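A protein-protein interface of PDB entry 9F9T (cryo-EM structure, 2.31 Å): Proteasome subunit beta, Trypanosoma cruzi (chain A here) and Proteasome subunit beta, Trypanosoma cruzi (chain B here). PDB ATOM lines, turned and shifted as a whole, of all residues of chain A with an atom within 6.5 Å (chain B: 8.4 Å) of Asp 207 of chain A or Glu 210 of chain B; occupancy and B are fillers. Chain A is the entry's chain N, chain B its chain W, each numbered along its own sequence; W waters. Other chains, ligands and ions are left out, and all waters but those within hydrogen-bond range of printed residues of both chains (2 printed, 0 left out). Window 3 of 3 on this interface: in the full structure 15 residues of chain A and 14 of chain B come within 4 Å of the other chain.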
ATOM      1  N   GLU A 205      25.944  25.858   1.978  1.00  0.00           N
ATOM      2  CA  GLU A 205      26.732  26.454   0.905  1.00  0.00           C
ATOM      3  C   GLU A 205      25.948  26.693  -0.365  1.00  0.00           C
ATOM      4  O   GLU A 205      26.520  27.043  -1.372  1.00  0.00           O
ATOM      5  CB  GLU A 205      27.985  25.633   0.598  1.00  0.00           C
ATOM      6  CG  GLU A 205      29.110  25.918   1.603  1.00  0.00           C
ATOM      7  CD  GLU A 205      29.950  24.705   1.950  1.00  0.00           C
ATOM      8  OE1 GLU A 205      29.396  23.558   1.907  1.00  0.00           O
ATOM      9  OE2 GLU A 205      31.130  24.901   2.309  1.00  0.00           O
ATOM     10  N   TYR A 206      24.648  26.639  -0.299  1.00  0.00           N
ATOM     11  CA  TYR A 206      23.852  26.923  -1.472  1.00  0.00           C
ATOM     12  C   TYR A 206      24.209  28.267  -2.075  1.00  0.00           C
ATOM     13  O   TYR A 206      24.430  29.252  -1.369  1.00  0.00           O
ATOM     14  CB  TYR A 206      22.414  26.908  -0.935  1.00  0.00           C
ATOM     15  CG  TYR A 206      21.929  25.619  -0.286  1.00  0.00           C
ATOM     16  CD1 TYR A 206      22.075  24.393  -0.909  1.00  0.00           C
ATOM     17  CD2 TYR A 206      21.310  25.631   0.957  1.00  0.00           C
ATOM     18  CE1 TYR A 206      21.644  23.205  -0.315  1.00  0.00           C
ATOM     19  CE2 TYR A 206      20.874  24.466   1.550  1.00  0.00           C
ATOM     20  CZ  TYR A 206      21.011  23.252   0.905  1.00  0.00           C
ATOM     21  OH  TYR A 206      20.548  22.112   1.474  1.00  0.00           O
ATOM     22  N   ASP A 207      24.165  28.358  -3.402  1.00  0.00           N
ATOM     23  CA  ASP A 207      24.282  29.650  -4.049  1.00  0.00           C
ATOM     24  C   ASP A 207      23.215  30.652  -3.571  1.00  0.00           C
ATOM     25  O   ASP A 207      23.474  31.839  -3.458  1.00  0.00           O
ATOM     26  CB  ASP A 207      24.194  29.549  -5.566  1.00  0.00           C
ATOM     27  CG  ASP A 207      23.829  30.902  -6.176  1.00  0.00           C
ATOM     28  OD1 ASP A 207      24.741  31.803  -6.241  1.00  0.00           O
ATOM     29  OD2 ASP A 207      22.599  31.095  -6.529  1.00  0.00           O
ATOM     30  N   GLY A 208      21.983  30.250  -3.312  1.00  0.00           N
ATOM     31  CA  GLY A 208      20.991  31.235  -2.846  1.00  0.00           C
ATOM     32  C   GLY A 208      21.280  31.822  -1.443  1.00  0.00           C
ATOM     33  O   GLY A 208      20.647  32.814  -1.072  1.00  0.00           O
ATOM     34  N   PHE A 209      22.258  31.247  -0.718  1.00  0.00           N
ATOM     35  CA  PHE A 209      22.703  31.769   0.551  1.00  0.00           C
ATOM     36  C   PHE A 209      23.893  32.711   0.442  1.00  0.00           C
ATOM     37  O   PHE A 209      24.367  33.238   1.434  1.00  0.00           O
ATOM     38  CB  PHE A 209      23.139  30.658   1.505  1.00  0.00           C
ATOM     39  CG  PHE A 209      22.033  29.833   2.105  1.00  0.00           C
ATOM     40  CD1 PHE A 209      20.707  30.033   1.744  1.00  0.00           C
ATOM     41  CD2 PHE A 209      22.345  28.874   3.044  1.00  0.00           C
ATOM     42  CE1 PHE A 209      19.687  29.286   2.293  1.00  0.00           C
ATOM     43  CE2 PHE A 209      21.311  28.130   3.630  1.00  0.00           C
ATOM     44  CZ  PHE A 209      19.966  28.357   3.260  1.00  0.00           C
ATOM     45  N   CYS A 210      24.362  32.982  -0.746  1.00  0.00           N
ATOM     46  CA  CYS A 210      25.505  33.844  -0.874  1.00  0.00           C
ATOM     47  C   CYS A 210      25.150  35.314  -0.598  1.00  0.00           C
ATOM     48  O   CYS A 210      24.004  35.703  -0.644  1.00  0.00           O
ATOM     49  CB  CYS A 210      26.101  33.736  -2.263  1.00  0.00           C
ATOM     50  SG  CYS A 210      25.096  34.570  -3.514  1.00  0.00           S
ATOM     51  N   PHE A 211      26.193  36.113  -0.333  1.00  0.00           N
ATOM     52  CA  PHE A 211      26.101  37.484   0.106  1.00  0.00           C
ATOM     53  C   PHE A 211      25.357  38.354  -0.906  1.00  0.00           C
ATOM     54  O   PHE A 211      24.528  39.150  -0.519  1.00  0.00           O
ATOM     55  CB  PHE A 211      27.531  37.966   0.385  1.00  0.00           C
ATOM     56  CG  PHE A 211      27.671  39.250   1.142  1.00  0.00           C
ATOM     57  CD1 PHE A 211      27.463  40.463   0.525  1.00  0.00           C
ATOM     58  CD2 PHE A 211      28.010  39.235   2.493  1.00  0.00           C
ATOM     59  CE1 PHE A 211      27.645  41.648   1.221  1.00  0.00           C
ATOM     60  CE2 PHE A 211      28.176  40.416   3.208  1.00  0.00           C
ATOM     61  CZ  PHE A 211      27.973  41.632   2.564  1.00  0.00           C
ATOM     62  N   LYS A 213      23.115  37.576  -3.321  1.00  0.00           N
ATOM     63  CA  LYS A 213      21.697  37.310  -3.481  1.00  0.00           C
ATOM     64  C   LYS A 213      20.884  37.654  -2.231  1.00  0.00           C
ATOM     65  O   LYS A 213      19.698  37.912  -2.344  1.00  0.00           O
ATOM     66  CB  LYS A 213      21.448  35.817  -3.650  1.00  0.00           C
ATOM     67  CG  LYS A 213      21.922  35.178  -4.940  1.00  0.00           C
ATOM     68  CD  LYS A 213      20.890  35.113  -6.053  1.00  0.00           C
ATOM     69  CE  LYS A 213      21.174  33.943  -6.967  1.00  0.00           C
ATOM     70  NZ  LYS A 213      20.690  34.238  -8.326  1.00  0.00           N
ATOM     71  N   THR A 214      21.466  37.616  -1.034  1.00  0.00           N
ATOM     72  CA  THR A 214      20.679  37.886   0.153  1.00  0.00           C
ATOM     73  C   THR A 214      20.754  39.350   0.618  1.00  0.00           C
ATOM     74  O   THR A 214      20.120  39.702   1.633  1.00  0.00           O
ATOM     75  CB  THR A 214      21.123  36.976   1.279  1.00  0.00           C
ATOM     76  OG1 THR A 214      22.522  37.229   1.289  1.00  0.00           O
ATOM     77  CG2 THR A 214      20.889  35.523   0.942  1.00  0.00           C
ATOM     78  N   VAL B  73      13.046  27.474  -5.923  1.00  0.00           N
ATOM     79  CA  VAL B  73      13.772  27.789  -7.136  1.00  0.00           C
ATOM     80  C   VAL B  73      14.391  26.505  -7.665  1.00  0.00           C
ATOM     81  O   VAL B  73      14.919  25.695  -6.909  1.00  0.00           O
ATOM     82  CB  VAL B  73      14.871  28.815  -6.788  1.00  0.00           C
ATOM     83  CG1 VAL B  73      15.785  29.108  -7.909  1.00  0.00           C
ATOM     84  CG2 VAL B  73      14.291  30.104  -6.343  1.00  0.00           C
ATOM     85  N   TYR B  74      14.334  26.329  -8.969  1.00  0.00           N
ATOM     86  CA  TYR B  74      15.009  25.223  -9.631  1.00  0.00           C
ATOM     87  C   TYR B  74      15.747  25.773 -10.836  1.00  0.00           C
ATOM     88  O   TYR B  74      15.761  26.988 -11.033  1.00  0.00           O
ATOM     89  CB  TYR B  74      14.036  24.126 -10.053  1.00  0.00           C
ATOM     90  CG  TYR B  74      13.123  24.435 -11.209  1.00  0.00           C
ATOM     91  CD1 TYR B  74      11.958  25.147 -11.038  1.00  0.00           C
ATOM     92  CD2 TYR B  74      13.384  23.924 -12.465  1.00  0.00           C
ATOM     93  CE1 TYR B  74      11.109  25.394 -12.118  1.00  0.00           C
ATOM     94  CE2 TYR B  74      12.584  24.215 -13.565  1.00  0.00           C
ATOM     95  CZ  TYR B  74      11.412  24.911 -13.379  1.00  0.00           C
ATOM     96  OH  TYR B  74      10.623  25.165 -14.459  1.00  0.00           O
ATOM     97  N   LYS B  75      16.451  24.903 -11.551  1.00  0.00           N
ATOM     98  CA  LYS B  75      17.435  25.326 -12.543  1.00  0.00           C
ATOM     99  C   LYS B  75      16.821  26.353 -13.485  1.00  0.00           C
ATOM    100  O   LYS B  75      17.414  27.386 -13.720  1.00  0.00           O
ATOM    101  CB  LYS B  75      17.947  24.110 -13.309  1.00  0.00           C
ATOM    102  CG  LYS B  75      19.438  24.079 -13.601  1.00  0.00           C
ATOM    103  CD  LYS B  75      19.925  25.088 -14.644  1.00  0.00           C
ATOM    104  CE  LYS B  75      21.000  24.536 -15.569  1.00  0.00           C
ATOM    105  NZ  LYS B  75      21.992  23.698 -14.851  1.00  0.00           N
ATOM    106  N   PRO B 174      15.319  33.536 -12.095  1.00  0.00           N
ATOM    107  CA  PRO B 174      14.296  33.227 -11.080  1.00  0.00           C
ATOM    108  C   PRO B 174      14.397  34.063  -9.816  1.00  0.00           C
ATOM    109  O   PRO B 174      15.499  34.286  -9.341  1.00  0.00           O
ATOM    110  CB  PRO B 174      14.672  31.791 -10.632  1.00  0.00           C
ATOM    111  CG  PRO B 174      15.377  31.278 -11.835  1.00  0.00           C
ATOM    112  CD  PRO B 174      16.238  32.418 -12.327  1.00  0.00           C
ATOM    113  N   ARG B 187      14.646  37.165   0.375  1.00  0.00           N
ATOM    114  CA  ARG B 187      14.831  36.392  -0.803  1.00  0.00           C
ATOM    115  C   ARG B 187      15.637  35.155  -0.471  1.00  0.00           C
ATOM    116  O   ARG B 187      16.701  35.267   0.108  1.00  0.00           O
ATOM    117  CB  ARG B 187      15.539  37.350  -1.757  1.00  0.00           C
ATOM    118  CG  ARG B 187      16.224  36.571  -2.855  1.00  0.00           C
ATOM    119  CD  ARG B 187      16.656  37.403  -4.033  1.00  0.00           C
ATOM    120  NE  ARG B 187      16.923  36.479  -5.129  1.00  0.00           N
ATOM    121  CZ  ARG B 187      17.254  36.888  -6.333  1.00  0.00           C
ATOM    122  NH1 ARG B 187      17.844  38.064  -6.483  1.00  0.00           N
ATOM    123  NH2 ARG B 187      17.077  36.078  -7.364  1.00  0.00           N
ATOM    124  N   LEU B 188      15.136  33.986  -0.836  1.00  0.00           N
ATOM    125  CA  LEU B 188      15.715  32.714  -0.425  1.00  0.00           C
ATOM    126  C   LEU B 188      15.455  31.643  -1.467  1.00  0.00           C
ATOM    127  O   LEU B 188      14.571  31.779  -2.280  1.00  0.00           O
ATOM    128  CB  LEU B 188      15.059  32.259   0.876  1.00  0.00           C
ATOM    129  CG  LEU B 188      15.534  32.957   2.135  1.00  0.00           C
ATOM    130  CD1 LEU B 188      14.755  32.463   3.333  1.00  0.00           C
ATOM    131  CD2 LEU B 188      17.026  32.706   2.335  1.00  0.00           C
ATOM    132  N   PRO B 189      16.238  30.577  -1.566  1.00  0.00           N
ATOM    133  CA  PRO B 189      15.981  29.522  -2.572  1.00  0.00           C
ATOM    134  C   PRO B 189      14.794  28.590  -2.297  1.00  0.00           C
ATOM    135  O   PRO B 189      14.351  27.890  -3.180  1.00  0.00           O
ATOM    136  CB  PRO B 189      17.337  28.712  -2.559  1.00  0.00           C
ATOM    137  CG  PRO B 189      17.833  28.878  -1.129  1.00  0.00           C
ATOM    138  CD  PRO B 189      17.488  30.356  -0.839  1.00  0.00           C
ATOM    139  N   PHE B 190      14.351  28.514  -1.059  1.00  0.00           N
ATOM    140  CA  PHE B 190      13.158  27.771  -0.707  1.00  0.00           C
ATOM    141  C   PHE B 190      12.503  28.441   0.484  1.00  0.00           C
ATOM    142  O   PHE B 190      13.210  28.917   1.321  1.00  0.00           O
ATOM    143  CB  PHE B 190      13.457  26.301  -0.424  1.00  0.00           C
ATOM    144  CG  PHE B 190      14.531  26.014   0.592  1.00  0.00           C
ATOM    145  CD1 PHE B 190      15.861  25.989   0.242  1.00  0.00           C
ATOM    146  CD2 PHE B 190      14.216  25.717   1.898  1.00  0.00           C
ATOM    147  CE1 PHE B 190      16.854  25.718   1.175  1.00  0.00           C
ATOM    148  CE2 PHE B 190      15.182  25.321   2.803  1.00  0.00           C
ATOM    149  CZ  PHE B 190      16.522  25.367   2.461  1.00  0.00           C
ATOM    150  N   GLY B 207      15.131  17.752   1.558  1.00  0.00           N
ATOM    151  CA  GLY B 207      14.999  17.359   0.174  1.00  0.00           C
ATOM    152  C   GLY B 207      15.479  18.382  -0.854  1.00  0.00           C
ATOM    153  O   GLY B 207      15.529  18.064  -2.026  1.00  0.00           O
ATOM    154  N   TYR B 208      15.725  19.635  -0.487  1.00  0.00           N
ATOM    155  CA  TYR B 208      16.205  20.593  -1.464  1.00  0.00           C
ATOM    156  C   TYR B 208      17.635  20.270  -1.793  1.00  0.00           C
ATOM    157  O   TYR B 208      18.381  19.771  -0.973  1.00  0.00           O
ATOM    158  CB  TYR B 208      16.152  22.004  -0.910  1.00  0.00           C
ATOM    159  CG  TYR B 208      16.703  23.091  -1.792  1.00  0.00           C
ATOM    160  CD1 TYR B 208      15.934  23.622  -2.799  1.00  0.00           C
ATOM    161  CD2 TYR B 208      18.010  23.553  -1.643  1.00  0.00           C
ATOM    162  CE1 TYR B 208      16.460  24.581  -3.670  1.00  0.00           C
ATOM    163  CE2 TYR B 208      18.553  24.488  -2.508  1.00  0.00           C
ATOM    164  CZ  TYR B 208      17.751  25.028  -3.503  1.00  0.00           C
ATOM    165  OH  TYR B 208      18.141  26.017  -4.349  1.00  0.00           O
ATOM    166  N   LYS B 209      17.963  20.484  -3.035  1.00  0.00           N
ATOM    167  CA  LYS B 209      19.336  20.558  -3.484  1.00  0.00           C
ATOM    168  C   LYS B 209      19.380  21.582  -4.602  1.00  0.00           C
ATOM    169  O   LYS B 209      18.347  22.146  -5.016  1.00  0.00           O
ATOM    170  CB  LYS B 209      19.809  19.195  -3.934  1.00  0.00           C
ATOM    171  CG  LYS B 209      19.022  18.604  -5.070  1.00  0.00           C
ATOM    172  CD  LYS B 209      19.296  17.099  -5.203  1.00  0.00           C
ATOM    173  CE  LYS B 209      18.575  16.477  -6.392  1.00  0.00           C
ATOM    174  NZ  LYS B 209      19.494  15.682  -7.242  1.00  0.00           N
ATOM    175  N   GLU B 210      20.615  21.862  -5.006  1.00  0.00           N
ATOM    176  CA  GLU B 210      20.875  22.830  -6.048  1.00  0.00           C
ATOM    177  C   GLU B 210      20.628  22.210  -7.418  1.00  0.00           C
ATOM    178  O   GLU B 210      20.829  21.013  -7.635  1.00  0.00           O
ATOM    179  CB  GLU B 210      22.296  23.365  -5.876  1.00  0.00           C
ATOM    180  CG  GLU B 210      22.357  24.676  -5.089  1.00  0.00           C
ATOM    181  CD  GLU B 210      23.733  25.323  -5.105  1.00  0.00           C
ATOM    182  OE1 GLU B 210      23.916  26.302  -5.870  1.00  0.00           O
ATOM    183  OE2 GLU B 210      24.632  24.835  -4.374  1.00  0.00           O
ATOM    184  N   ASN B 211      20.118  23.071  -8.314  1.00  0.00           N
ATOM    185  CA  ASN B 211      19.915  22.782  -9.733  1.00  0.00           C
ATOM    186  C   ASN B 211      19.102  21.499  -9.951  1.00  0.00           C
ATOM    187  O   ASN B 211      19.354  20.742 -10.895  1.00  0.00           O
ATOM    188  CB  ASN B 211      21.256  22.785 -10.468  1.00  0.00           C
ATOM    189  CG  ASN B 211      21.813  24.189 -10.563  1.00  0.00           C
ATOM    190  OD1 ASN B 211      21.068  25.169 -10.655  1.00  0.00           O
ATOM    191  ND2 ASN B 211      23.127  24.294 -10.464  1.00  0.00           N
ATOM    192  N   MET B 212      18.129  21.291  -9.052  1.00  0.00           N
ATOM    193  CA  MET B 212      16.971  20.450  -9.244  1.00  0.00           C
ATOM    194  C   MET B 212      16.408  20.664 -10.638  1.00  0.00           C
ATOM    195  O   MET B 212      16.347  21.803 -11.102  1.00  0.00           O
ATOM    196  CB  MET B 212      15.890  20.897  -8.253  1.00  0.00           C
ATOM    197  CG  MET B 212      16.013  20.206  -6.930  1.00  0.00           C
ATOM    198  SD  MET B 212      14.699  20.457  -5.757  1.00  0.00           S
ATOM    199  CE  MET B 212      14.642  22.238  -5.701  1.00  0.00           C
ATOM    200  N   THR B 213      15.920  19.586 -11.235  1.00  0.00           N
ATOM    201  CA  THR B 213      15.126  19.614 -12.460  1.00  0.00           C
ATOM    202  C   THR B 213      13.672  19.970 -12.163  1.00  0.00           C
ATOM    203  O   THR B 213      13.238  19.919 -11.023  1.00  0.00           O
ATOM    204  CB  THR B 213      15.089  18.211 -13.074  1.00  0.00           C
ATOM    205  OG1 THR B 213      14.477  17.348 -12.104  1.00  0.00           O
ATOM    206  CG2 THR B 213      16.474  17.710 -13.411  1.00  0.00           C
ATOM    207  N   GLU B 216      11.888  16.932 -10.104  1.00  0.00           N
ATOM    208  CA  GLU B 216      12.307  16.942  -8.713  1.00  0.00           C
ATOM    209  C   GLU B 216      11.718  18.109  -7.904  1.00  0.00           C
ATOM    210  O   GLU B 216      11.439  17.946  -6.719  1.00  0.00           O
ATOM    211  CB  GLU B 216      13.818  17.058  -8.688  1.00  0.00           C
ATOM    212  CG  GLU B 216      14.534  15.836  -9.223  1.00  0.00           C
ATOM    213  CD  GLU B 216      16.054  16.008  -9.202  1.00  0.00           C
ATOM    214  OE1 GLU B 216      16.538  17.099  -9.664  1.00  0.00           O
ATOM    215  OE2 GLU B 216      16.759  15.046  -8.766  1.00  0.00           O
HETATM  216  O   HOH W   1      20.672  27.510  -4.267  1.00  0.00           O
HETATM  217  O   HOH W   2      18.566  34.013  -1.841  1.00  0.00           O
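Printed residues of chain B within 4 Å of Tyr 206 of chain A: Tyr 208 (3.9 Å) and Glu 210 (3.7 Å).
Of chain B, only Glu 210 comes within 4 Å of Asp 207 of chain A.
Gly 208 of chain A touches none of the printed residues of chain B.
Printed residues of chain B within 4 Å of Phe 209 of chain A: Pro 189 (3.9 Å).
Printed residues of chain A within 4 Å of Arg 187 of chain B: Lys 213 (3.5 Å).
The nearest residue of chain B that does not touch Asp 207 of chain A is Pro 189 of chain B (6.2 Å).
Of the 9 printed residues of chain A, 4 touch a printed residue of chain B.
Hydrophobic or aromatic side chains of chain A that line the printed part of chain B: Tyr 206 and Phe 209.
Along chain B the printed residues that touch a printed residue of chain A span positions 187 to 210.
Among the printed residues, no Asp or Glu carboxylate lies within 4 Å of a Lys or Arg side-chain nitrogen of the other chain.
Water W2 lies within hydrogen-bond range of the backbone carbonyl oxygen (O) of Gly 208 of chain A (2.5 Å) and the backbone carbonyl oxygen (O) of Arg 187 of chain B (3.0 Å).
Water W1 bridges OH of Tyr 208 of chain B (2.9 Å) and N of Gly 208 of chain A (3.2 Å).
The backbone NH of Asp 207 of chain A sits at hydrogen-bond distance from the side-chain carboxylate of Glu 210 of chain B.
O of Asp 207 of chain A is in hydrogen-bond range of SG of Cys 210 of chain A (3.2 Å).
The side-chain sulfur (SG) of Cys 210 of chain A lies close to the backbone NH (N) of Lys 213 of chain A, 3.6 Å away.
The backbone NH (N) of Val 73 of chain B sits at hydrogen-bond distance from the backbone carbonyl oxygen (O) of Pro 189 of chain B (3.1 Å).
The backbone carbonyl oxygen of Pro 174 of chain B sits at hydrogen-bond distance from the guanidinium group of Arg 187 of chain B (3.1 Å).
Tyr 208 of chain B touches Tyr 206 of chain A.
OE2 of Glu 210 of chain B touches CA of Tyr 206 of chain A, 3.7 Å away.
CE1 of Phe 209 of chain A touches CG of Pro 189 of chain B, at 3.9 Å.
O of Lys 213 of chain A touches CD of Arg 187 of chain B, at 3.5 Å.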
